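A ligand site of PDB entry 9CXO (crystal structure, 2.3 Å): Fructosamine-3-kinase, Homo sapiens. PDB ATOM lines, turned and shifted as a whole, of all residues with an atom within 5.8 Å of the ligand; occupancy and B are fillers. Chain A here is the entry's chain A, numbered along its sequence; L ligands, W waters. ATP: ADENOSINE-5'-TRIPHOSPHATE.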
ATOM      1  N   GLY A  22       6.176  16.556  14.143  1.00  0.00           N
ATOM      2  CA  GLY A  22       6.434  15.696  15.287  1.00  0.00           C
ATOM      3  C   GLY A  22       6.486  14.233  14.897  1.00  0.00           C
ATOM      4  O   GLY A  22       5.769  13.766  14.003  1.00  0.00           O
ATOM      5  N   ALA A  23       7.361  13.496  15.571  1.00  0.00           N
ATOM      6  CA  ALA A  23       7.637  12.096  15.219  1.00  0.00           C
ATOM      7  C   ALA A  23       6.663  11.198  15.990  1.00  0.00           C
ATOM      8  O   ALA A  23       7.044  10.415  16.859  1.00  0.00           O
ATOM      9  CB  ALA A  23       9.093  11.746  15.501  1.00  0.00           C
ATOM     10  N   GLY A  24       5.390  11.346  15.643  1.00  0.00           N
ATOM     11  CA  GLY A  24       4.337  10.569  16.253  1.00  0.00           C
ATOM     12  C   GLY A  24       3.824   9.473  15.327  1.00  0.00           C
ATOM     13  O   GLY A  24       3.668   9.674  14.126  1.00  0.00           O
ATOM     14  N   CYS A  25       3.572   8.304  15.917  1.00  0.00           N
ATOM     15  CA  CYS A  25       2.911   7.207  15.230  1.00  0.00           C
ATOM     16  C   CYS A  25       1.406   7.297  15.357  1.00  0.00           C
ATOM     17  O   CYS A  25       0.675   7.015  14.400  1.00  0.00           O
ATOM     18  CB  CYS A  25       3.417   5.862  15.766  1.00  0.00           C
ATOM     19  SG  CYS A  25       2.538   4.414  15.136  1.00  0.00           S
ATOM     20  N   ILE A  26       0.916   7.689  16.538  1.00  0.00           N
ATOM     21  CA  ILE A  26      -0.516   7.756  16.774  1.00  0.00           C
ATOM     22  C   ILE A  26      -1.113   8.941  16.022  1.00  0.00           C
ATOM     23  O   ILE A  26      -2.111   8.814  15.308  1.00  0.00           O
ATOM     24  CB  ILE A  26      -0.816   7.875  18.276  1.00  0.00           C
ATOM     25  CG1 ILE A  26      -0.409   6.617  19.059  1.00  0.00           C
ATOM     26  CG2 ILE A  26      -2.280   8.231  18.505  1.00  0.00           C
ATOM     27  CD1 ILE A  26      -0.739   5.289  18.432  1.00  0.00           C
ATOM     28  N   SER A  27      -0.498  10.114  16.171  1.00  0.00           N
ATOM     29  CA  SER A  27      -1.064  11.363  15.670  1.00  0.00           C
ATOM     30  C   SER A  27       0.009  12.197  14.993  1.00  0.00           C
ATOM     31  O   SER A  27       1.210  11.892  15.067  1.00  0.00           O
ATOM     32  CB  SER A  27      -1.722  12.165  16.801  1.00  0.00           C
ATOM     33  OG  SER A  27      -2.711  11.404  17.470  1.00  0.00           O
ATOM     34  N   GLU A  28      -0.434  13.246  14.319  1.00  0.00           N
ATOM     35  CA  GLU A  28       0.444  14.207  13.667  1.00  0.00           C
ATOM     36  C   GLU A  28       0.688  15.385  14.610  1.00  0.00           C
ATOM     37  O   GLU A  28      -0.265  15.992  15.104  1.00  0.00           O
ATOM     38  CB  GLU A  28      -0.152  14.697  12.356  1.00  0.00           C
ATOM     39  N   GLY A  29       1.955  15.684  14.851  1.00  0.00           N
ATOM     40  CA  GLY A  29       2.297  16.730  15.791  1.00  0.00           C
ATOM     41  C   GLY A  29       3.013  17.903  15.152  1.00  0.00           C
ATOM     42  O   GLY A  29       3.954  17.727  14.376  1.00  0.00           O
ATOM     43  N   PHE A  40       2.227  22.940  21.456  1.00  0.00           N
ATOM     44  CA  PHE A  40       2.338  21.739  20.635  1.00  0.00           C
ATOM     45  C   PHE A  40       0.940  21.173  20.413  1.00  0.00           C
ATOM     46  O   PHE A  40       0.149  21.084  21.357  1.00  0.00           O
ATOM     47  CB  PHE A  40       3.237  20.693  21.295  1.00  0.00           C
ATOM     48  CG  PHE A  40       3.606  19.550  20.396  1.00  0.00           C
ATOM     49  CD1 PHE A  40       4.566  19.713  19.416  1.00  0.00           C
ATOM     50  CD2 PHE A  40       2.975  18.323  20.519  1.00  0.00           C
ATOM     51  CE1 PHE A  40       4.902  18.664  18.586  1.00  0.00           C
ATOM     52  CE2 PHE A  40       3.312  17.274  19.690  1.00  0.00           C
ATOM     53  CZ  PHE A  40       4.275  17.445  18.717  1.00  0.00           C
ATOM     54  N   LYS A  42      -1.393  18.061  18.671  1.00  0.00           N
ATOM     55  CA  LYS A  42      -1.527  16.725  18.107  1.00  0.00           C
ATOM     56  C   LYS A  42      -2.886  16.612  17.435  1.00  0.00           C
ATOM     57  O   LYS A  42      -3.909  16.955  18.035  1.00  0.00           O
ATOM     58  CB  LYS A  42      -1.364  15.647  19.187  1.00  0.00           C
ATOM     59  CG  LYS A  42       0.043  15.551  19.763  1.00  0.00           C
ATOM     60  CD  LYS A  42       0.338  14.145  20.269  1.00  0.00           C
ATOM     61  CE  LYS A  42      -0.345  13.890  21.600  1.00  0.00           C
ATOM     62  NZ  LYS A  42       0.042  12.566  22.173  1.00  0.00           N
ATOM     63  N   PHE A  53      -7.974  11.467  23.329  1.00  0.00           N
ATOM     64  CA  PHE A  53      -7.274  12.629  23.855  1.00  0.00           C
ATOM     65  C   PHE A  53      -7.770  12.999  25.257  1.00  0.00           C
ATOM     66  O   PHE A  53      -6.982  13.493  26.075  1.00  0.00           O
ATOM     67  CB  PHE A  53      -7.436  13.822  22.913  1.00  0.00           C
ATOM     68  CG  PHE A  53      -6.543  13.754  21.704  1.00  0.00           C
ATOM     69  CD1 PHE A  53      -5.252  13.269  21.812  1.00  0.00           C
ATOM     70  CD2 PHE A  53      -6.996  14.183  20.476  1.00  0.00           C
ATOM     71  CE1 PHE A  53      -4.427  13.204  20.708  1.00  0.00           C
ATOM     72  CE2 PHE A  53      -6.169  14.124  19.364  1.00  0.00           C
ATOM     73  CZ  PHE A  53      -4.889  13.637  19.481  1.00  0.00           C
ATOM     74  N   GLU A  56      -5.955  10.901  27.570  1.00  0.00           N
ATOM     75  CA  GLU A  56      -4.601  11.426  27.704  1.00  0.00           C
ATOM     76  C   GLU A  56      -4.577  12.653  28.613  1.00  0.00           C
ATOM     77  O   GLU A  56      -3.645  12.819  29.409  1.00  0.00           O
ATOM     78  CB  GLU A  56      -4.020  11.758  26.329  1.00  0.00           C
ATOM     79  CG  GLU A  56      -2.551  12.159  26.352  1.00  0.00           C
ATOM     80  CD  GLU A  56      -1.983  12.381  24.960  1.00  0.00           C
ATOM     81  OE1 GLU A  56      -2.613  11.926  23.980  1.00  0.00           O
ATOM     82  OE2 GLU A  56      -0.905  13.011  24.850  1.00  0.00           O
ATOM     83  N   PRO A  72       3.841  17.881  30.053  1.00  0.00           N
ATOM     84  CA  PRO A  72       3.251  19.064  29.436  1.00  0.00           C
ATOM     85  C   PRO A  72       1.854  19.327  29.968  1.00  0.00           C
ATOM     86  O   PRO A  72       1.075  18.406  30.199  1.00  0.00           O
ATOM     87  CB  PRO A  72       3.232  18.723  27.937  1.00  0.00           C
ATOM     88  CG  PRO A  72       4.122  17.521  27.780  1.00  0.00           C
ATOM     89  CD  PRO A  72       4.077  16.795  29.084  1.00  0.00           C
ATOM     90  N   MET A  89      -1.405  21.442  23.920  1.00  0.00           N
ATOM     91  CA  MET A  89      -0.750  21.385  25.212  1.00  0.00           C
ATOM     92  C   MET A  89       0.436  22.338  25.204  1.00  0.00           C
ATOM     93  O   MET A  89       0.854  22.850  24.162  1.00  0.00           O
ATOM     94  CB  MET A  89      -0.279  19.958  25.549  1.00  0.00           C
ATOM     95  CG  MET A  89       0.996  19.534  24.833  1.00  0.00           C
ATOM     96  SD  MET A  89       1.020  17.769  24.434  1.00  0.00           S
ATOM     97  CE  MET A  89       0.711  17.065  26.056  1.00  0.00           C
ATOM     98  N   GLU A  90       0.968  22.601  26.396  1.00  0.00           N
ATOM     99  CA  GLU A  90       2.147  23.436  26.541  1.00  0.00           C
ATOM    100  C   GLU A  90       3.322  22.828  25.775  1.00  0.00           C
ATOM    101  O   GLU A  90       3.573  21.619  25.845  1.00  0.00           O
ATOM    102  CB  GLU A  90       2.503  23.598  28.013  1.00  0.00           C
ATOM    103  CG  GLU A  90       3.958  23.923  28.302  1.00  0.00           C
ATOM    104  CD  GLU A  90       4.331  23.687  29.750  1.00  0.00           C
ATOM    105  OE1 GLU A  90       3.705  22.813  30.387  1.00  0.00           O
ATOM    106  OE2 GLU A  90       5.252  24.367  30.253  1.00  0.00           O
ATOM    107  N   HIS A  91       4.033  23.667  25.012  1.00  0.00           N
ATOM    108  CA  HIS A  91       5.204  23.201  24.298  1.00  0.00           C
ATOM    109  C   HIS A  91       6.409  23.141  25.222  1.00  0.00           C
ATOM    110  O   HIS A  91       6.629  24.044  26.035  1.00  0.00           O
ATOM    111  CB  HIS A  91       5.515  24.107  23.103  1.00  0.00           C
ATOM    112  CG  HIS A  91       6.769  23.738  22.373  1.00  0.00           C
ATOM    113  ND1 HIS A  91       8.012  24.193  22.752  1.00  0.00           N
ATOM    114  CD2 HIS A  91       6.967  22.944  21.290  1.00  0.00           C
ATOM    115  CE1 HIS A  91       8.928  23.704  21.931  1.00  0.00           C
ATOM    116  NE2 HIS A  91       8.316  22.940  21.031  1.00  0.00           N
ATOM    117  N   LEU A  92       7.186  22.079  25.098  1.00  0.00           N
ATOM    118  CA  LEU A  92       8.377  21.872  25.907  1.00  0.00           C
ATOM    119  C   LEU A  92       9.565  21.632  25.000  1.00  0.00           C
ATOM    120  O   LEU A  92       9.530  20.735  24.152  1.00  0.00           O
ATOM    121  CB  LEU A  92       8.188  20.694  26.868  1.00  0.00           C
ATOM    122  CG  LEU A  92       7.161  20.896  27.991  1.00  0.00           C
ATOM    123  CD1 LEU A  92       6.960  19.612  28.764  1.00  0.00           C
ATOM    124  CD2 LEU A  92       7.601  22.023  28.921  1.00  0.00           C
ATOM    125  N   LYS A  93      10.612  22.431  25.171  1.00  0.00           N
ATOM    126  CA  LYS A  93      11.884  22.149  24.507  1.00  0.00           C
ATOM    127  C   LYS A  93      12.464  20.869  25.093  1.00  0.00           C
ATOM    128  O   LYS A  93      12.726  20.793  26.296  1.00  0.00           O
ATOM    129  CB  LYS A  93      12.847  23.320  24.686  1.00  0.00           C
ATOM    130  N   MET A  94      12.664  19.860  24.245  1.00  0.00           N
ATOM    131  CA  MET A  94      12.975  18.522  24.719  1.00  0.00           C
ATOM    132  C   MET A  94      14.151  17.944  23.952  1.00  0.00           C
ATOM    133  O   MET A  94      14.359  18.235  22.770  1.00  0.00           O
ATOM    134  CB  MET A  94      11.758  17.596  24.580  1.00  0.00           C
ATOM    135  CG  MET A  94      10.601  17.961  25.494  1.00  0.00           C
ATOM    136  SD  MET A  94       9.249  16.786  25.373  1.00  0.00           S
ATOM    137  CE  MET A  94       9.278  16.440  23.630  1.00  0.00           C
ATOM    138  N   TRP A 201       7.809   4.025  27.438  1.00  0.00           N
ATOM    139  CA  TRP A 201       8.909   3.647  26.563  1.00  0.00           C
ATOM    140  C   TRP A 201       9.769   4.858  26.224  1.00  0.00           C
ATOM    141  O   TRP A 201       9.367   6.006  26.395  1.00  0.00           O
ATOM    142  CB  TRP A 201       8.405   2.939  25.298  1.00  0.00           C
ATOM    143  CG  TRP A 201       7.833   3.816  24.214  1.00  0.00           C
ATOM    144  CD1 TRP A 201       6.661   4.514  24.253  1.00  0.00           C
ATOM    145  CD2 TRP A 201       8.374   4.016  22.903  1.00  0.00           C
ATOM    146  NE1 TRP A 201       6.460   5.180  23.069  1.00  0.00           N
ATOM    147  CE2 TRP A 201       7.503   4.896  22.218  1.00  0.00           C
ATOM    148  CE3 TRP A 201       9.534   3.566  22.239  1.00  0.00           C
ATOM    149  CZ2 TRP A 201       7.749   5.324  20.908  1.00  0.00           C
ATOM    150  CZ3 TRP A 201       9.771   3.998  20.930  1.00  0.00           C
ATOM    151  CH2 TRP A 201       8.876   4.867  20.282  1.00  0.00           C
ATOM    152  N   GLY A 203      10.526   6.391  23.689  1.00  0.00           N
ATOM    153  CA  GLY A 203       9.932   7.391  22.823  1.00  0.00           C
ATOM    154  C   GLY A 203       9.013   8.364  23.529  1.00  0.00           C
ATOM    155  O   GLY A 203       8.675   9.392  22.933  1.00  0.00           O
ATOM    156  N   ASN A 204       8.594   8.080  24.762  1.00  0.00           N
ATOM    157  CA  ASN A 204       7.676   8.947  25.486  1.00  0.00           C
ATOM    158  C   ASN A 204       8.343   9.697  26.645  1.00  0.00           C
ATOM    159  O   ASN A 204       7.636  10.299  27.460  1.00  0.00           O
ATOM    160  CB  ASN A 204       6.485   8.137  26.015  1.00  0.00           C
ATOM    161  CG  ASN A 204       5.471   7.818  24.933  1.00  0.00           C
ATOM    162  OD1 ASN A 204       5.383   8.518  23.931  1.00  0.00           O
ATOM    163  ND2 ASN A 204       4.706   6.752  25.140  1.00  0.00           N
ATOM    164  N   TYR A 215       5.671  12.162  28.764  1.00  0.00           N
ATOM    165  CA  TYR A 215       4.488  12.633  28.059  1.00  0.00           C
ATOM    166  C   TYR A 215       3.790  11.439  27.414  1.00  0.00           C
ATOM    167  O   TYR A 215       4.265  10.299  27.485  1.00  0.00           O
ATOM    168  CB  TYR A 215       4.870  13.688  27.010  1.00  0.00           C
ATOM    169  CG  TYR A 215       5.997  13.251  26.093  1.00  0.00           C
ATOM    170  CD1 TYR A 215       5.737  12.482  24.967  1.00  0.00           C
ATOM    171  CD2 TYR A 215       7.316  13.592  26.371  1.00  0.00           C
ATOM    172  CE1 TYR A 215       6.760  12.070  24.135  1.00  0.00           C
ATOM    173  CE2 TYR A 215       8.343  13.187  25.546  1.00  0.00           C
ATOM    174  CZ  TYR A 215       8.064  12.425  24.421  1.00  0.00           C
ATOM    175  OH  TYR A 215       9.082  12.024  23.596  1.00  0.00           O
ATOM    176  N   ASP A 216       2.638  11.711  26.791  1.00  0.00           N
ATOM    177  CA  ASP A 216       1.818  10.732  26.091  1.00  0.00           C
ATOM    178  C   ASP A 216       1.437   9.568  26.995  1.00  0.00           C
ATOM    179  O   ASP A 216       1.602   8.404  26.609  1.00  0.00           O
ATOM    180  CB  ASP A 216       2.557  10.219  24.852  1.00  0.00           C
ATOM    181  CG  ASP A 216       1.631   9.548  23.859  1.00  0.00           C
ATOM    182  OD1 ASP A 216       0.413   9.821  23.901  1.00  0.00           O
ATOM    183  OD2 ASP A 216       2.121   8.736  23.046  1.00  0.00           O
HETATM  184  PG  ATP L   1       3.535   7.779  19.789  1.00  0.00           P
HETATM  185  O1G ATP L   1       2.912   6.689  18.986  1.00  0.00           O
HETATM  186  O2G ATP L   1       4.078   7.313  21.146  1.00  0.00           O
HETATM  187  O3G ATP L   1       4.645   8.531  19.041  1.00  0.00           O
HETATM  188  PB  ATP L   1       1.800  10.203  19.504  1.00  0.00           P
HETATM  189  O1B ATP L   1       1.677  10.106  18.033  1.00  0.00           O
HETATM  190  O2B ATP L   1       0.493  10.467  20.262  1.00  0.00           O
HETATM  191  O3B ATP L   1       2.451   8.904  20.134  1.00  0.00           O
HETATM  192  PA  ATP L   1       3.664  11.715  21.234  1.00  0.00           P
HETATM  193  O1A ATP L   1       4.392  10.539  21.763  1.00  0.00           O
HETATM  194  O2A ATP L   1       2.701  12.381  22.216  1.00  0.00           O
HETATM  195  O3A ATP L   1       2.838  11.335  19.926  1.00  0.00           O
HETATM  196  O5' ATP L   1       4.668  12.808  20.689  1.00  0.00           O
HETATM  197  C5' ATP L   1       5.455  12.585  19.507  1.00  0.00           C
HETATM  198  C4' ATP L   1       6.626  13.528  19.500  1.00  0.00           C
HETATM  199  O4' ATP L   1       6.147  14.887  19.479  1.00  0.00           O
HETATM  200  C3' ATP L   1       7.542  13.459  20.709  1.00  0.00           C
HETATM  201  O3' ATP L   1       8.518  12.436  20.554  1.00  0.00           O
HETATM  202  C2' ATP L   1       8.175  14.854  20.715  1.00  0.00           C
HETATM  203  O2' ATP L   1       9.271  14.943  19.805  1.00  0.00           O
HETATM  204  C1' ATP L   1       7.009  15.723  20.244  1.00  0.00           C
HETATM  205  N9  ATP L   1       6.232  16.326  21.320  1.00  0.00           N
HETATM  206  C8  ATP L   1       5.196  15.762  22.021  1.00  0.00           C
HETATM  207  N7  ATP L   1       4.683  16.529  22.937  1.00  0.00           N
HETATM  208  C5  ATP L   1       5.422  17.697  22.849  1.00  0.00           C
HETATM  209  C6  ATP L   1       5.383  18.907  23.551  1.00  0.00           C
HETATM  210  N6  ATP L   1       4.514  19.173  24.532  1.00  0.00           N
HETATM  211  N1  ATP L   1       6.270  19.869  23.211  1.00  0.00           N
HETATM  212  C2  ATP L   1       7.134  19.620  22.230  1.00  0.00           C
HETATM  213  N3  ATP L   1       7.279  18.510  21.495  1.00  0.00           N
HETATM  214  C4  ATP L   1       6.385  17.583  21.850  1.00  0.00           C
HETATM  215  O   HOH W   1       2.761  14.649  24.068  1.00  0.00           O
HETATM  216  O   HOH W   2      -1.854  10.989  20.192  1.00  0.00           O
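Merely in contact with the ligand: Gly 24, Phe 40, His 91, Met 94, Pro 72, Trp 201, Ala 23 and Gly 203. Hydrophobic or aromatic side chains within 4 Å of the ligand: Ile 26, Phe 40, Pro 72, Met 89, His 91, Met 94 and Tyr 215.
The backbone NH (N) of Ile 26 lies within hydrogen-bond range of an oxygen (O1B) of the ligand, at 2.9 Å. An oxygen (O2A) of the ligand lies within salt-bridge range of the side-chain amino group of Lys 42. A nitrogen (N6) of the ligand lies within hydrogen-bond range of the backbone carbonyl oxygen (O) of Glu 90, at 2.9 Å. A nitrogen (N6) of the ligand lies close to the side-chain sulfur (SD) of Met 89. N of Cys 25 lies within hydrogen-bond range of O3G of the ligand, 3.3 Å away. An oxygen (O1B) of the ligand sits at hydrogen-bond distance from the backbone NH (N) of Ser 27, 2.9 Å away. The side-chain carboxylate (OD2) of Asp 216 sits close to an oxygen (O2G) of the ligand, at 3.1 Å. The side-chain amide oxygen of Asn 204 lies close to an oxygen (O1A) of the ligand. The backbone NH (N) of Leu 92 is in hydrogen-bond range of a nitrogen (N1) of the ligand (3.0 Å). The side-chain hydroxyl of Tyr 215 is in hydrogen-bond range of an oxygen (O3') of the ligand (3.1 Å).
Water W2 lies within hydrogen-bond range of an oxygen (O2B) of the ligand (2.4 Å), the side-chain hydroxyl (OG) of Ser 27 (2.9 Å) and the side-chain amino group (NZ) of Lys 42 (3.2 Å). Water W1 bridges N7 of the ligand (2.9 Å) and SD of Met 89 (3.6 Å).
O of Asn 204 sits at hydrogen-bond distance from N of Tyr 215 (3.0 Å). The side-chain carboxylate (OD2) of Asp 216 sits close to the side-chain amide oxygen (OD1) of Asn 204. O of Phe 40 lies within hydrogen-bond range of N of Met 89, at 3.0 Å. The side-chain amino group (NZ) of Lys 42 is in salt-bridge range of the side-chain carboxylate (OD1) of Asp 216 (3.3 Å). The side-chain hydroxyl (OH) of Tyr 215 sits at hydrogen-bond distance from the backbone carbonyl oxygen (O) of Gly 203, at 2.7 Å. The side-chain amino group (NZ) of Lys 42 is in salt-bridge range of the side-chain carboxylate (OE2) of Glu 56, 2.9 Å away. NE1 of Trp 201 sits close to ND2 of Asn 204, at 3.1 Å.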
